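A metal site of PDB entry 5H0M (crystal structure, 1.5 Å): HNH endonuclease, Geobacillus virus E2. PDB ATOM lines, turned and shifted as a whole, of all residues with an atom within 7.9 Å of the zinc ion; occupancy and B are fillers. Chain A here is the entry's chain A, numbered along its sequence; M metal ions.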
ATOM      1  N   LEU A  75     -22.866  -9.463  -1.508  1.00  0.00           N
ATOM      2  CA  LEU A  75     -22.780  -8.000  -1.580  1.00  0.00           C
ATOM      3  C   LEU A  75     -21.683  -7.432  -0.717  1.00  0.00           C
ATOM      4  O   LEU A  75     -21.464  -7.871   0.408  1.00  0.00           O
ATOM      5  CB  LEU A  75     -24.097  -7.363  -1.137  1.00  0.00           C
ATOM      6  CG  LEU A  75     -25.301  -7.675  -2.013  1.00  0.00           C
ATOM      7  CD1 LEU A  75     -26.515  -6.990  -1.425  1.00  0.00           C
ATOM      8  CD2 LEU A  75     -25.063  -7.230  -3.446  1.00  0.00           C
ATOM      9  N   CYS A  76     -21.010  -6.412  -1.233  1.00  0.00           N
ATOM     10  CA  CYS A  76     -20.015  -5.675  -0.451  1.00  0.00           C
ATOM     11  C   CYS A  76     -20.675  -5.036   0.746  1.00  0.00           C
ATOM     12  O   CYS A  76     -21.587  -4.237   0.604  1.00  0.00           O
ATOM     13  CB  CYS A  76     -19.337  -4.619  -1.293  1.00  0.00           C
ATOM     14  SG  CYS A  76     -18.187  -3.596  -0.352  1.00  0.00           S
ATOM     15  N   GLN A  77     -20.202  -5.381   1.947  1.00  0.00           N
ATOM     16  CA  GLN A  77     -20.817  -4.886   3.188  1.00  0.00           C
ATOM     17  C   GLN A  77     -20.490  -3.443   3.495  1.00  0.00           C
ATOM     18  O   GLN A  77     -21.268  -2.772   4.167  1.00  0.00           O
ATOM     19  CB  GLN A  77     -20.453  -5.815   4.355  1.00  0.00           C
ATOM     20  CG  GLN A  77     -20.951  -7.236   4.156  1.00  0.00           C
ATOM     21  CD  GLN A  77     -22.462  -7.302   4.023  1.00  0.00           C
ATOM     22  OE1 GLN A  77     -23.011  -7.603   2.951  1.00  0.00           O
ATOM     23  NE2 GLN A  77     -23.149  -6.987   5.093  1.00  0.00           N
ATOM     24  N   HIS A  78     -19.369  -2.947   3.009  1.00  0.00           N
ATOM     25  CA  HIS A  78     -19.057  -1.527   3.195  1.00  0.00           C
ATOM     26  C   HIS A  78     -19.902  -0.670   2.286  1.00  0.00           C
ATOM     27  O   HIS A  78     -20.472   0.314   2.729  1.00  0.00           O
ATOM     28  CB  HIS A  78     -17.580  -1.281   2.988  1.00  0.00           C
ATOM     29  CG  HIS A  78     -16.731  -1.846   4.068  1.00  0.00           C
ATOM     30  ND1 HIS A  78     -15.423  -1.463   4.252  1.00  0.00           N
ATOM     31  CD2 HIS A  78     -17.015  -2.727   5.054  1.00  0.00           C
ATOM     32  CE1 HIS A  78     -14.931  -2.110   5.297  1.00  0.00           C
ATOM     33  NE2 HIS A  78     -15.876  -2.886   5.792  1.00  0.00           N
ATOM     34  N   CYS A  79     -20.023  -1.071   1.028  1.00  0.00           N
ATOM     35  CA  CYS A  79     -20.926  -0.382   0.110  1.00  0.00           C
ATOM     36  C   CYS A  79     -22.349  -0.406   0.647  1.00  0.00           C
ATOM     37  O   CYS A  79     -23.038   0.619   0.606  1.00  0.00           O
ATOM     38  CB  CYS A  79     -20.877  -1.034  -1.269  1.00  0.00           C
ATOM     39  SG  CYS A  79     -19.488  -0.569  -2.334  1.00  0.00           S
ATOM     40  N   LEU A  80     -22.789  -1.537   1.169  1.00  0.00           N
ATOM     41  CA  LEU A  80     -24.169  -1.632   1.672  1.00  0.00           C
ATOM     42  C   LEU A  80     -24.411  -0.617   2.807  1.00  0.00           C
ATOM     43  O   LEU A  80     -25.463   0.039   2.848  1.00  0.00           O
ATOM     44  CB  LEU A  80     -24.464  -3.057   2.157  1.00  0.00           C
ATOM     45  CG  LEU A  80     -25.932  -3.407   2.427  1.00  0.00           C
ATOM     46  CD1 LEU A  80     -26.773  -3.284   1.166  1.00  0.00           C
ATOM     47  CD2 LEU A  80     -26.023  -4.806   3.005  1.00  0.00           C
ATOM     48  N   GLU A  82     -22.957   2.156   3.158  1.00  0.00           N
ATOM     49  CA  GLU A  82     -22.986   3.447   2.465  1.00  0.00           C
ATOM     50  C   GLU A  82     -24.137   3.559   1.481  1.00  0.00           C
ATOM     51  O   GLU A  82     -24.134   4.436   0.614  1.00  0.00           O
ATOM     52  CB  GLU A  82     -21.647   3.665   1.743  1.00  0.00           C
ATOM     53  CG  GLU A  82     -20.491   3.754   2.718  1.00  0.00           C
ATOM     54  CD  GLU A  82     -19.159   3.941   2.016  1.00  0.00           C
ATOM     55  OE1 GLU A  82     -18.881   3.197   1.064  1.00  0.00           O
ATOM     56  OE2 GLU A  82     -18.396   4.827   2.445  1.00  0.00           O
ATOM     57  N   LYS A  84     -25.158   1.561  -1.049  1.00  0.00           N
ATOM     58  CA  LYS A  84     -24.766   1.212  -2.398  1.00  0.00           C
ATOM     59  C   LYS A  84     -24.790  -0.291  -2.567  1.00  0.00           C
ATOM     60  O   LYS A  84     -24.545  -1.034  -1.610  1.00  0.00           O
ATOM     61  CB  LYS A  84     -23.356   1.746  -2.686  1.00  0.00           C
ATOM     62  CG  LYS A  84     -23.270   3.267  -2.713  1.00  0.00           C
ATOM     63  CD  LYS A  84     -21.854   3.776  -2.523  1.00  0.00           C
ATOM     64  CE  LYS A  84     -20.975   3.346  -3.681  1.00  0.00           C
ATOM     65  NZ  LYS A  84     -19.651   4.013  -3.565  1.00  0.00           N
ATOM     66  N   ILE A  85     -25.068  -0.727  -3.784  1.00  0.00           N
ATOM     67  CA  ILE A  85     -25.129  -2.139  -4.145  1.00  0.00           C
ATOM     68  C   ILE A  85     -23.973  -2.483  -5.068  1.00  0.00           C
ATOM     69  O   ILE A  85     -23.910  -2.025  -6.219  1.00  0.00           O
ATOM     70  CB  ILE A  85     -26.457  -2.496  -4.824  1.00  0.00           C
ATOM     71  CG1 ILE A  85     -27.633  -2.221  -3.890  1.00  0.00           C
ATOM     72  CG2 ILE A  85     -26.457  -3.945  -5.281  1.00  0.00           C
ATOM     73  CD1 ILE A  85     -27.631  -2.981  -2.577  1.00  0.00           C
ATOM     74  N   THR A  86     -23.047  -3.312  -4.562  1.00  0.00           N
ATOM     75  CA  THR A  86     -21.867  -3.717  -5.310  1.00  0.00           C
ATOM     76  C   THR A  86     -21.572  -5.178  -5.030  1.00  0.00           C
ATOM     77  O   THR A  86     -21.561  -5.599  -3.872  1.00  0.00           O
ATOM     78  CB  THR A  86     -20.633  -2.900  -4.911  1.00  0.00           C
ATOM     79  OG1 THR A  86     -20.958  -1.501  -4.932  1.00  0.00           O
ATOM     80  CG2 THR A  86     -19.492  -3.172  -5.867  1.00  0.00           C
ATOM     81  N   ARG A  87     -21.325  -5.936  -6.079  1.00  0.00           N
ATOM     82  CA  ARG A  87     -20.944  -7.334  -5.936  1.00  0.00           C
ATOM     83  C   ARG A  87     -19.614  -7.452  -5.173  1.00  0.00           C
ATOM     84  O   ARG A  87     -18.649  -6.776  -5.504  1.00  0.00           O
ATOM     85  CB  ARG A  87     -20.780  -7.971  -7.307  1.00  0.00           C
ATOM     86  CG  ARG A  87     -20.361  -9.425  -7.267  1.00  0.00           C
ATOM     87  CD  ARG A  87     -21.558 -10.316  -7.424  1.00  0.00           C
ATOM     88  NE  ARG A  87     -21.198 -11.725  -7.430  1.00  0.00           N
ATOM     89  CZ  ARG A  87     -22.079 -12.721  -7.381  1.00  0.00           C
ATOM     90  NH1 ARG A  87     -23.382 -12.447  -7.301  1.00  0.00           N
ATOM     91  NH2 ARG A  87     -21.672 -13.982  -7.379  1.00  0.00           N
ATOM     92  N   ALA A  88     -19.571  -8.328  -4.182  1.00  0.00           N
ATOM     93  CA  ALA A  88     -18.323  -8.630  -3.485  1.00  0.00           C
ATOM     94  C   ALA A  88     -17.432  -9.538  -4.317  1.00  0.00           C
ATOM     95  O   ALA A  88     -17.932 -10.423  -5.005  1.00  0.00           O
ATOM     96  CB  ALA A  88     -18.601  -9.288  -2.159  1.00  0.00           C
ATOM     97  N   SER A 112     -17.500  -9.552   3.336  1.00  0.00           N
ATOM     98  CA  SER A 112     -17.433  -9.580   1.888  1.00  0.00           C
ATOM     99  C   SER A 112     -17.276  -8.147   1.381  1.00  0.00           C
ATOM    100  O   SER A 112     -18.013  -7.265   1.822  1.00  0.00           O
ATOM    101  CB  SER A 112     -18.725 -10.165   1.321  1.00  0.00           C
ATOM    102  OG  SER A 112     -19.009 -11.444   1.884  1.00  0.00           O
ATOM    103  N   LEU A 113     -16.311  -7.933   0.480  1.00  0.00           N
ATOM    104  CA  LEU A 113     -15.937  -6.591  -0.006  1.00  0.00           C
ATOM    105  C   LEU A 113     -15.757  -6.571  -1.504  1.00  0.00           C
ATOM    106  O   LEU A 113     -15.343  -7.571  -2.100  1.00  0.00           O
ATOM    107  CB  LEU A 113     -14.635  -6.100   0.626  1.00  0.00           C
ATOM    108  CG  LEU A 113     -14.588  -5.962   2.159  1.00  0.00           C
ATOM    109  CD1 LEU A 113     -13.207  -5.514   2.587  1.00  0.00           C
ATOM    110  CD2 LEU A 113     -15.649  -4.988   2.651  1.00  0.00           C
ATOM    111  N   CYS A 114     -16.059  -5.424  -2.108  1.00  0.00           N
ATOM    112  CA  CYS A 114     -15.670  -5.150  -3.481  1.00  0.00           C
ATOM    113  C   CYS A 114     -14.200  -4.743  -3.502  1.00  0.00           C
ATOM    114  O   CYS A 114     -13.568  -4.534  -2.464  1.00  0.00           O
ATOM    115  CB  CYS A 114     -16.547  -4.056  -4.093  1.00  0.00           C
ATOM    116  SG  CYS A 114     -16.242  -2.388  -3.481  1.00  0.00           S
ATOM    117  N   GLN A 115     -13.614  -4.647  -4.681  1.00  0.00           N
ATOM    118  CA  GLN A 115     -12.201  -4.304  -4.776  1.00  0.00           C
ATOM    119  C   GLN A 115     -11.908  -2.912  -4.230  1.00  0.00           C
ATOM    120  O   GLN A 115     -10.910  -2.702  -3.542  1.00  0.00           O
ATOM    121  CB  GLN A 115     -11.729  -4.390  -6.228  1.00  0.00           C
ATOM    122  CG  GLN A 115     -10.341  -3.820  -6.428  1.00  0.00           C
ATOM    123  CD  GLN A 115      -9.862  -3.979  -7.835  1.00  0.00           C
ATOM    124  OE1 GLN A 115     -10.360  -4.830  -8.572  1.00  0.00           O
ATOM    125  NE2 GLN A 115      -8.870  -3.182  -8.205  1.00  0.00           N
ATOM    126  N   ALA A 116     -12.741  -1.936  -4.561  1.00  0.00           N
ATOM    127  CA  ALA A 116     -12.531  -0.575  -4.112  1.00  0.00           C
ATOM    128  C   ALA A 116     -12.550  -0.473  -2.599  1.00  0.00           C
ATOM    129  O   ALA A 116     -11.728   0.211  -2.000  1.00  0.00           O
ATOM    130  CB  ALA A 116     -13.536   0.383  -4.727  1.00  0.00           C
ATOM    131  N   CYS A 117     -13.497  -1.175  -1.977  1.00  0.00           N
ATOM    132  CA  CYS A 117     -13.573  -1.187  -0.520  1.00  0.00           C
ATOM    133  C   CYS A 117     -12.417  -1.952   0.106  1.00  0.00           C
ATOM    134  O   CYS A 117     -11.931  -1.577   1.154  1.00  0.00           O
ATOM    135  CB  CYS A 117     -14.915  -1.723  -0.052  1.00  0.00           C
ATOM    136  SG  CYS A 117     -16.249  -0.534  -0.370  1.00  0.00           S
ATOM    137  N   HIS A 118     -11.952  -3.012  -0.535  1.00  0.00           N
ATOM    138  CA  HIS A 118     -10.768  -3.722  -0.034  1.00  0.00           C
ATOM    139  C   HIS A 118      -9.533  -2.822  -0.090  1.00  0.00           C
ATOM    140  O   HIS A 118      -8.726  -2.786   0.841  1.00  0.00           O
ATOM    141  CB  HIS A 118     -10.524  -5.005  -0.817  1.00  0.00           C
ATOM    142  CG  HIS A 118      -9.378  -5.806  -0.283  1.00  0.00           C
ATOM    143  ND1 HIS A 118      -8.164  -5.866  -0.925  1.00  0.00           N
ATOM    144  CD2 HIS A 118      -9.251  -6.561   0.841  1.00  0.00           C
ATOM    145  CE1 HIS A 118      -7.341  -6.641  -0.232  1.00  0.00           C
ATOM    146  NE2 HIS A 118      -7.970  -7.069   0.843  1.00  0.00           N
ATOM    147  N   ARG A 120      -9.560   0.524  -0.023  1.00  0.00           N
ATOM    148  CA  ARG A 120      -9.742   1.531   1.007  1.00  0.00           C
ATOM    149  C   ARG A 120      -9.385   0.973   2.372  1.00  0.00           C
ATOM    150  O   ARG A 120      -8.699   1.613   3.160  1.00  0.00           O
ATOM    151  CB  ARG A 120     -11.195   2.056   1.010  1.00  0.00           C
ATOM    152  CG  ARG A 120     -11.525   2.962   2.176  1.00  0.00           C
ATOM    153  CD  ARG A 120     -12.867   3.630   2.053  1.00  0.00           C
ATOM    154  NE  ARG A 120     -13.975   2.683   1.937  1.00  0.00           N
ATOM    155  CZ  ARG A 120     -15.264   3.024   1.875  1.00  0.00           C
ATOM    156  NH1 ARG A 120     -15.630   4.300   1.926  1.00  0.00           N
ATOM    157  NH2 ARG A 120     -16.196   2.088   1.774  1.00  0.00           N
HETATM  158 ZN    ZN M   1     -17.673  -1.805  -1.709  1.00  0.00          ZN
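SG of Cys 117 lies close to NH2 of Arg 120 (3.4 Å). The side-chain sulfur (SG) of Cys 76 lies close to the backbone NH (N) of His 78, 3.6 Å away. SG of Cys 114 lies close to N of Ala 116, at 3.7 Å. The backbone NH (N) of Lys 84 sits at hydrogen-bond distance from the backbone carbonyl oxygen (O) of Cys 79 (2.8 Å). The side-chain sulfur of Cys 79 sits close to the side-chain hydroxyl of Thr 86 (3.1 Å). N of Cys 76 is in hydrogen-bond range of O of Thr 86.
The zinc ion is bound by the side-chain sulfur of Cys 79 (2.3 Å), the side-chain sulfur of Cys 76 (2.3 Å), the side-chain sulfur of Cys 117 (2.3 Å) and the side-chain sulfur of Cys 114 (2.4 Å).
Within 4 Å of the zinc ion: Cys 76, Cys 79, Cys 114 and Cys 117.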
